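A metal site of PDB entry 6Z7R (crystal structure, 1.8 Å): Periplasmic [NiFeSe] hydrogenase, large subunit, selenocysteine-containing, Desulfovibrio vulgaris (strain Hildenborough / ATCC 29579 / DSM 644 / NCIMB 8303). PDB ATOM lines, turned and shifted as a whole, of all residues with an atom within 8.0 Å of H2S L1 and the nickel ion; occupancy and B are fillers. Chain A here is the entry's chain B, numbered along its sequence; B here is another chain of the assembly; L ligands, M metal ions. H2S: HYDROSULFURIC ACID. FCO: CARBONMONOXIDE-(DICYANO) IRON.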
ATOM      1  N   GLU A  17     -25.536  13.603   8.314  1.00  0.00           N
ATOM      2  CA  GLU A  17     -24.660  12.824   7.450  1.00  0.00           C
ATOM      3  C   GLU A  17     -23.270  12.714   8.070  1.00  0.00           C
ATOM      4  O   GLU A  17     -22.733  13.682   8.595  1.00  0.00           O
ATOM      5  CB  GLU A  17     -24.535  13.467   6.080  1.00  0.00           C
ATOM      6  CG  GLU A  17     -23.769  12.678   5.036  1.00  0.00           C
ATOM      7  CD  GLU A  17     -22.253  12.550   5.295  1.00  0.00           C
ATOM      8  OE1 GLU A  17     -21.669  13.456   5.881  1.00  0.00           O
ATOM      9  OE2 GLU A  17     -21.667  11.520   4.909  1.00  0.00           O
ATOM     10  N   GLN A  61     -17.144  14.442  -6.175  1.00  0.00           N
ATOM     11  CA  GLN A  61     -18.526  14.294  -5.788  1.00  0.00           C
ATOM     12  C   GLN A  61     -18.669  13.255  -4.699  1.00  0.00           C
ATOM     13  O   GLN A  61     -19.630  13.322  -3.907  1.00  0.00           O
ATOM     14  CB  GLN A  61     -19.378  13.943  -7.011  1.00  0.00           C
ATOM     15  CG  GLN A  61     -19.649  15.112  -7.976  1.00  0.00           C
ATOM     16  CD  GLN A  61     -20.635  14.725  -9.014  1.00  0.00           C
ATOM     17  OE1 GLN A  61     -21.858  14.646  -8.762  1.00  0.00           O
ATOM     18  NE2 GLN A  61     -20.129  14.455 -10.185  1.00  0.00           N
ATOM     19  N   ILE A  63     -16.988  12.905  -2.183  1.00  0.00           N
ATOM     20  CA  ILE A  63     -16.900  13.469  -0.854  1.00  0.00           C
ATOM     21  C   ILE A  63     -18.222  13.324  -0.139  1.00  0.00           C
ATOM     22  O   ILE A  63     -18.206  13.044   1.032  1.00  0.00           O
ATOM     23  CB  ILE A  63     -16.445  14.933  -0.944  1.00  0.00           C
ATOM     24  CG1 ILE A  63     -14.950  14.962  -1.319  1.00  0.00           C
ATOM     25  CG2 ILE A  63     -16.786  15.781   0.300  1.00  0.00           C
ATOM     26  CD1 ILE A  63     -14.477  16.251  -1.792  1.00  0.00           C
ATOM     27  N   CSD A  64     -19.352  13.525  -0.839  1.00  0.00           N
ATOM     28  CA  CSD A  64     -20.637  13.554  -0.190  1.00  0.00           C
ATOM     29  CB  CSD A  64     -20.896  14.966   0.354  1.00  0.00           C
ATOM     30  SG  CSD A  64     -21.955  15.022   1.765  1.00  0.00           S
ATOM     31  C   CSD A  64     -21.739  13.187  -1.169  1.00  0.00           C
ATOM     32  O   CSD A  64     -21.947  13.861  -2.177  1.00  0.00           O
ATOM     33  OD1 CSD A  64     -21.011  14.710   2.824  1.00  0.00           O
ATOM     34  N   GLY A  65     -22.458  12.107  -0.870  1.00  0.00           N
ATOM     35  CA  GLY A  65     -23.531  11.643  -1.735  1.00  0.00           C
ATOM     36  C   GLY A  65     -24.841  12.389  -1.549  1.00  0.00           C
ATOM     37  O   GLY A  65     -25.773  12.220  -2.344  1.00  0.00           O
ATOM     38  N   VAL A  66     -24.903  13.247  -0.526  1.00  0.00           N
ATOM     39  CA  VAL A  66     -26.051  14.106  -0.298  1.00  0.00           C
ATOM     40  C   VAL A  66     -25.924  15.424  -1.055  1.00  0.00           C
ATOM     41  O   VAL A  66     -26.923  15.933  -1.555  1.00  0.00           O
ATOM     42  CB  VAL A  66     -26.243  14.383   1.200  1.00  0.00           C
ATOM     43  CG1 VAL A  66     -27.458  15.310   1.445  1.00  0.00           C
ATOM     44  CG2 VAL A  66     -26.426  13.081   2.001  1.00  0.00           C
ATOM     45  N   CYS A  67     -24.721  16.028  -1.092  1.00  0.00           N
ATOM     46  CA  CYS A  67     -24.443  17.249  -1.836  1.00  0.00           C
ATOM     47  C   CYS A  67     -23.424  17.103  -2.958  1.00  0.00           C
ATOM     48  O   CYS A  67     -22.613  18.011  -3.161  1.00  0.00           O
ATOM     49  CB  CYS A  67     -23.948  18.329  -0.872  1.00  0.00           C
ATOM     50  SG  CYS A  67     -22.274  18.097  -0.196  1.00  0.00           S
ATOM     51  N   PRO A  68     -23.484  16.060  -3.790  1.00  0.00           N
ATOM     52  CA  PRO A  68     -22.432  15.899  -4.796  1.00  0.00           C
ATOM     53  C   PRO A  68     -22.478  16.966  -5.863  1.00  0.00           C
ATOM     54  O   PRO A  68     -21.414  17.362  -6.343  1.00  0.00           O
ATOM     55  CB  PRO A  68     -22.683  14.505  -5.374  1.00  0.00           C
ATOM     56  CG  PRO A  68     -24.081  14.275  -5.150  1.00  0.00           C
ATOM     57  CD  PRO A  68     -24.481  14.995  -3.888  1.00  0.00           C
ATOM     58  N   ALA A  70     -23.005  20.153  -5.401  1.00  0.00           N
ATOM     59  CA  ALA A  70     -22.248  21.332  -4.971  1.00  0.00           C
ATOM     60  C   ALA A  70     -20.757  21.200  -5.279  1.00  0.00           C
ATOM     61  O   ALA A  70     -20.153  22.114  -5.832  1.00  0.00           O
ATOM     62  CB  ALA A  70     -22.496  21.573  -3.493  1.00  0.00           C
ATOM     63  N   HIS A  71     -20.149  20.052  -4.965  1.00  0.00           N
ATOM     64  CA  HIS A  71     -18.727  19.810  -5.276  1.00  0.00           C
ATOM     65  C   HIS A  71     -18.468  19.751  -6.773  1.00  0.00           C
ATOM     66  O   HIS A  71     -17.443  20.256  -7.248  1.00  0.00           O
ATOM     67  CB  HIS A  71     -18.280  18.511  -4.606  1.00  0.00           C
ATOM     68  CG  HIS A  71     -18.290  18.587  -3.101  1.00  0.00           C
ATOM     69  ND1 HIS A  71     -17.391  19.357  -2.404  1.00  0.00           N
ATOM     70  CD2 HIS A  71     -19.121  18.042  -2.183  1.00  0.00           C
ATOM     71  CE1 HIS A  71     -17.665  19.270  -1.106  1.00  0.00           C
ATOM     72  NE2 HIS A  71     -18.708  18.474  -0.954  1.00  0.00           N
ATOM     73  N   ASN A 102     -31.134  19.896  -6.764  1.00  0.00           N
ATOM     74  CA  ASN A 102     -30.710  19.212  -5.566  1.00  0.00           C
ATOM     75  C   ASN A 102     -30.810  20.083  -4.316  1.00  0.00           C
ATOM     76  O   ASN A 102     -30.813  19.551  -3.200  1.00  0.00           O
ATOM     77  CB  ASN A 102     -29.265  18.681  -5.664  1.00  0.00           C
ATOM     78  CG  ASN A 102     -28.999  17.553  -4.653  1.00  0.00           C
ATOM     79  OD1 ASN A 102     -29.807  16.626  -4.549  1.00  0.00           O
ATOM     80  ND2 ASN A 102     -27.888  17.642  -3.876  1.00  0.00           N
ATOM     81  N   SER A 106     -32.236  18.400  -1.144  1.00  0.00           N
ATOM     82  CA  SER A 106     -31.461  18.410   0.099  1.00  0.00           C
ATOM     83  C   SER A 106     -32.233  19.076   1.226  1.00  0.00           C
ATOM     84  O   SER A 106     -32.245  18.574   2.358  1.00  0.00           O
ATOM     85  CB  SER A 106     -30.124  19.109  -0.119  1.00  0.00           C
ATOM     86  OG  SER A 106     -29.465  19.157   1.110  1.00  0.00           O
ATOM     87  N   LEU A 109     -35.077  16.579   2.190  1.00  0.00           N
ATOM     88  CA  LEU A 109     -34.444  15.498   2.943  1.00  0.00           C
ATOM     89  C   LEU A 109     -34.149  15.921   4.364  1.00  0.00           C
ATOM     90  O   LEU A 109     -34.447  15.190   5.327  1.00  0.00           O
ATOM     91  CB  LEU A 109     -33.148  15.077   2.236  1.00  0.00           C
ATOM     92  CG  LEU A 109     -32.365  14.006   2.990  1.00  0.00           C
ATOM     93  CD1 LEU A 109     -33.071  12.716   2.869  1.00  0.00           C
ATOM     94  CD2 LEU A 109     -30.967  13.864   2.464  1.00  0.00           C
ATOM     95  N   LEU A 114     -34.312  13.979   8.293  1.00  0.00           N
ATOM     96  CA  LEU A 114     -33.291  14.080   9.314  1.00  0.00           C
ATOM     97  C   LEU A 114     -33.788  14.743  10.585  1.00  0.00           C
ATOM     98  O   LEU A 114     -33.635  14.167  11.658  1.00  0.00           O
ATOM     99  CB  LEU A 114     -32.064  14.807   8.761  1.00  0.00           C
ATOM    100  CG  LEU A 114     -31.381  14.100   7.581  1.00  0.00           C
ATOM    101  CD1 LEU A 114     -30.103  14.739   7.102  1.00  0.00           C
ATOM    102  CD2 LEU A 114     -31.025  12.675   7.925  1.00  0.00           C
ATOM    103  N   ALA A 409     -23.176  25.427  -1.339  1.00  0.00           N
ATOM    104  CA  ALA A 409     -23.794  24.130  -1.200  1.00  0.00           C
ATOM    105  C   ALA A 409     -25.047  24.292  -0.361  1.00  0.00           C
ATOM    106  O   ALA A 409     -25.206  25.267   0.369  1.00  0.00           O
ATOM    107  CB  ALA A 409     -22.843  23.147  -0.563  1.00  0.00           C
ATOM    108  N   PRO A 410     -25.965  23.354  -0.447  1.00  0.00           N
ATOM    109  CA  PRO A 410     -27.148  23.460   0.404  1.00  0.00           C
ATOM    110  C   PRO A 410     -26.829  23.809   1.825  1.00  0.00           C
ATOM    111  O   PRO A 410     -27.618  24.472   2.487  1.00  0.00           O
ATOM    112  CB  PRO A 410     -27.735  22.057   0.275  1.00  0.00           C
ATOM    113  CG  PRO A 410     -27.444  21.743  -1.161  1.00  0.00           C
ATOM    114  CD  PRO A 410     -26.089  22.273  -1.420  1.00  0.00           C
ATOM    115  N   ARG A 411     -25.664  23.396   2.338  1.00  0.00           N
ATOM    116  CA  ARG A 411     -25.406  23.664   3.743  1.00  0.00           C
ATOM    117  C   ARG A 411     -24.523  24.857   3.950  1.00  0.00           C
ATOM    118  O   ARG A 411     -24.346  25.294   5.098  1.00  0.00           O
ATOM    119  CB  ARG A 411     -24.792  22.425   4.431  1.00  0.00           C
ATOM    120  CG  ARG A 411     -25.843  21.336   4.593  1.00  0.00           C
ATOM    121  CD  ARG A 411     -25.313  19.975   4.450  1.00  0.00           C
ATOM    122  NE  ARG A 411     -26.396  19.006   4.455  1.00  0.00           N
ATOM    123  CZ  ARG A 411     -27.067  18.688   3.365  1.00  0.00           C
ATOM    124  NH1 ARG A 411     -26.763  19.215   2.213  1.00  0.00           N
ATOM    125  NH2 ARG A 411     -28.060  17.854   3.424  1.00  0.00           N
ATOM    126  N   LEU A 414     -18.874  27.018  -0.179  1.00  0.00           N
ATOM    127  CA  LEU A 414     -18.015  25.981  -0.745  1.00  0.00           C
ATOM    128  C   LEU A 414     -17.056  26.620  -1.724  1.00  0.00           C
ATOM    129  O   LEU A 414     -17.473  27.438  -2.562  1.00  0.00           O
ATOM    130  CB  LEU A 414     -18.870  24.911  -1.416  1.00  0.00           C
ATOM    131  CG  LEU A 414     -18.138  23.814  -2.187  1.00  0.00           C
ATOM    132  CD1 LEU A 414     -17.098  23.147  -1.274  1.00  0.00           C
ATOM    133  CD2 LEU A 414     -19.060  22.688  -2.727  1.00  0.00           C
ATOM    134  N   SER A 432     -15.315  23.591   2.578  1.00  0.00           N
ATOM    135  CA  SER A 432     -16.730  23.233   2.451  1.00  0.00           C
ATOM    136  C   SER A 432     -17.622  23.785   3.570  1.00  0.00           C
ATOM    137  O   SER A 432     -17.167  24.310   4.590  1.00  0.00           O
ATOM    138  CB  SER A 432     -16.836  21.728   2.432  1.00  0.00           C
ATOM    139  OG  SER A 432     -16.459  21.209   3.689  1.00  0.00           O
ATOM    140  N   ALA A 433     -18.925  23.626   3.379  1.00  0.00           N
ATOM    141  CA  ALA A 433     -19.887  24.293   4.258  1.00  0.00           C
ATOM    142  C   ALA A 433     -19.793  23.763   5.685  1.00  0.00           C
ATOM    143  O   ALA A 433     -19.575  24.521   6.651  1.00  0.00           O
ATOM    144  CB  ALA A 433     -21.301  24.068   3.733  1.00  0.00           C
ATOM    145  N   SER A 434     -19.963  22.464   5.851  1.00  0.00           N
ATOM    146  CA  SER A 434     -19.909  21.933   7.224  1.00  0.00           C
ATOM    147  C   SER A 434     -18.507  21.993   7.847  1.00  0.00           C
ATOM    148  O   SER A 434     -18.367  21.742   9.036  1.00  0.00           O
ATOM    149  CB  SER A 434     -20.415  20.486   7.247  1.00  0.00           C
ATOM    150  OG  SER A 434     -21.781  20.524   6.879  1.00  0.00           O
ATOM    151  N   ASP A 476     -27.786  21.223   9.905  1.00  0.00           N
ATOM    152  CA  ASP A 476     -27.766  20.291   8.766  1.00  0.00           C
ATOM    153  C   ASP A 476     -26.356  19.806   8.459  1.00  0.00           C
ATOM    154  O   ASP A 476     -25.923  19.857   7.298  1.00  0.00           O
ATOM    155  CB  ASP A 476     -28.363  20.977   7.534  1.00  0.00           C
ATOM    156  CG  ASP A 476     -28.708  19.992   6.370  1.00  0.00           C
ATOM    157  OD1 ASP A 476     -28.598  18.750   6.502  1.00  0.00           O
ATOM    158  OD2 ASP A 476     -29.132  20.480   5.294  1.00  0.00           O
ATOM    159  N   PRO A 477     -25.632  19.264   9.454  1.00  0.00           N
ATOM    160  CA  PRO A 477     -24.242  18.871   9.277  1.00  0.00           C
ATOM    161  C   PRO A 477     -24.017  17.675   8.354  1.00  0.00           C
ATOM    162  O   PRO A 477     -24.838  16.759   8.275  1.00  0.00           O
ATOM    163  CB  PRO A 477     -23.780  18.508  10.706  1.00  0.00           C
ATOM    164  CG  PRO A 477     -24.948  18.606  11.579  1.00  0.00           C
ATOM    165  CD  PRO A 477     -26.151  18.812  10.762  1.00  0.00           C
ATOM    166  N   SEC A 478     -22.952  17.696   7.561  1.00  0.00           N
ATOM    167  CA  SEC A 478     -22.518  16.476   6.900  1.00  0.00           C
ATOM    168  CB  SEC A 478     -22.970  16.306   5.449  1.00  0.00           C
ATOM    169 SE   SEC A 478     -22.766  17.798   4.205  1.00  0.00          SE
ATOM    170  C   SEC A 478     -21.036  16.443   6.995  1.00  0.00           C
ATOM    171  O   SEC A 478     -20.348  17.329   6.482  1.00  0.00           O
ATOM    172  N   LEU A 479     -20.548  15.416   7.670  1.00  0.00           N
ATOM    173  CA  LEU A 479     -19.163  15.308   8.087  1.00  0.00           C
ATOM    174  C   LEU A 479     -18.308  14.792   6.971  1.00  0.00           C
ATOM    175  O   LEU A 479     -17.090  15.030   6.944  1.00  0.00           O
ATOM    176  CB  LEU A 479     -19.003  14.454   9.373  1.00  0.00           C
ATOM    177  CG  LEU A 479     -19.133  15.252  10.679  1.00  0.00           C
ATOM    178  CD1 LEU A 479     -17.956  16.166  10.768  1.00  0.00           C
ATOM    179  CD2 LEU A 479     -20.386  16.125  10.785  1.00  0.00           C
ATOM    180  N   GLY A 480     -18.933  14.176   5.977  1.00  0.00           N
ATOM    181  CA  GLY A 480     -18.177  13.827   4.795  1.00  0.00           C
ATOM    182  C   GLY A 480     -17.600  15.051   4.146  1.00  0.00           C
ATOM    183  O   GLY A 480     -16.419  15.081   3.805  1.00  0.00           O
ATOM    184  N   CYS A 481     -18.442  16.072   3.977  1.00  0.00           N
ATOM    185  CA  CYS A 481     -17.992  17.348   3.433  1.00  0.00           C
ATOM    186  C   CYS A 481     -17.018  18.045   4.356  1.00  0.00           C
ATOM    187  O   CYS A 481     -16.127  18.766   3.867  1.00  0.00           O
ATOM    188  CB  CYS A 481     -19.178  18.291   3.235  1.00  0.00           C
ATOM    189  SG  CYS A 481     -20.093  17.966   1.752  1.00  0.00           S
ATOM    190  N   ALA A 482     -17.207  17.930   5.685  1.00  0.00           N
ATOM    191  CA  ALA A 482     -16.363  18.723   6.607  1.00  0.00           C
ATOM    192  C   ALA A 482     -14.911  18.238   6.576  1.00  0.00           C
ATOM    193  O   ALA A 482     -13.975  19.043   6.617  1.00  0.00           O
ATOM    194  CB  ALA A 482     -16.920  18.731   8.044  1.00  0.00           C
ATOM    195  N   CYS B  18     -19.658   8.046   1.632  1.00  0.00           N
ATOM    196  CA  CYS B  18     -20.153   9.412   1.404  1.00  0.00           C
ATOM    197  C   CYS B  18     -21.661   9.504   1.654  1.00  0.00           C
ATOM    198  O   CYS B  18     -22.277  10.568   1.429  1.00  0.00           O
ATOM    199  CB  CYS B  18     -19.768   9.873  -0.006  1.00  0.00           C
ATOM    200  SG  CYS B  18     -20.790   9.258  -1.295  1.00  0.00           S
ATOM    201  N   THR B  19     -22.287   8.435   2.172  1.00  0.00           N
ATOM    202  CA  THR B  19     -23.741   8.334   2.357  1.00  0.00           C
ATOM    203  C   THR B  19     -24.480   8.224   1.006  1.00  0.00           C
ATOM    204  O   THR B  19     -25.714   8.172   0.972  1.00  0.00           O
ATOM    205  CB  THR B  19     -24.306   9.517   3.172  1.00  0.00           C
ATOM    206  OG1 THR B  19     -23.556   9.647   4.380  1.00  0.00           O
ATOM    207  CG2 THR B  19     -25.704   9.273   3.579  1.00  0.00           C
HETATM  208  S   H2S L   1     -24.103  17.284   2.577  1.00  0.00           S
HETATM  209 FE   FCO L   2     -21.755  19.568   1.464  1.00  0.00          FE
HETATM  210  C1  FCO L   2     -21.543  20.307   3.098  1.00  0.00           C
HETATM  211  N1  FCO L   2     -21.440  20.785   4.124  1.00  0.00           N
HETATM  212  C2  FCO L   2     -23.360  20.382   1.357  1.00  0.00           C
HETATM  213  N2  FCO L   2     -24.355  20.984   1.302  1.00  0.00           N
HETATM  214  C3  FCO L   2     -20.753  20.886   0.769  1.00  0.00           C
HETATM  215  O3  FCO L   2     -20.094  21.738   0.388  1.00  0.00           O
HETATM  216 NI    NI M   1     -22.187  17.329   2.023  1.00  0.00          NI
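The nickel ion is bound by S of H2S L1 (2.0 Å), SG of Cys 481 (2.2 Å), SE of SEC 478 (2.3 Å), SG of CSD 64 (2.3 Å) and SG of Cys 67 (2.3 Å).
The nickel ion has five donor atoms within binding distance.
Four residues have an atom within 4 Å of the nickel ion: CSD 64, Cys 67, SEC 478 and Cys 481.
Residues that only touch H2S L1: Val 66.
Hydrophobic or aromatic side chains within 4 Å of H2S L1: Val 66.
Within 4 Å of H2S L1: CSD 64, Val 66, Cys 67, Arg 411 and SEC 478.
A sulfur (S) of H2S L1 is bonded to SE of SEC 478, at 2.2 Å.
The guanidinium group of Arg 411 sits close to a sulfur (S) of H2S L1 (3.3 Å).
SG of Cys 481 binds FE of FCO L2 (2.3 Å).
FE of FCO L2 is bound by SG of Cys 67.
The backbone NH (N) of Arg 411 lies within hydrogen-bond range of a nitrogen (N2) of FCO L2 (2.9 Å).
The guanidinium group (NH1) of Arg 411 sits at hydrogen-bond distance from a nitrogen (N2) of FCO L2 (3.1 Å).
N of Ser 434 lies within hydrogen-bond range of N1 of FCO L2, 2.8 Å away.
The side-chain hydroxyl (OG) of Ser 434 sits at hydrogen-bond distance from a nitrogen (N1) of FCO L2, 2.8 Å away.
N of SEC 478 is in hydrogen-bond range of the side-chain hydroxyl of Ser 434 (3.1 Å).
SG of Cys 481 lies close to NE2 of His 71 (3.1 Å).
The backbone carbonyl oxygen of Cys 481 sits at hydrogen-bond distance from the side-chain hydroxyl of Ser 432.
A ring nitrogen (NE2) of His 71 lies close to the side-chain sulfur of Cys 67 (3.7 Å).
The guanidinium group (NE) of Arg 411 lies within salt-bridge range of the side-chain carboxylate (OD1) of Asp 476, at 3.0 Å.
OG of Ser 106 sits at hydrogen-bond distance from NH1 of Arg 411, at 2.9 Å.
O of Val 66 lies within hydrogen-bond range of ND2 of Asn 102, at 3.0 Å.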
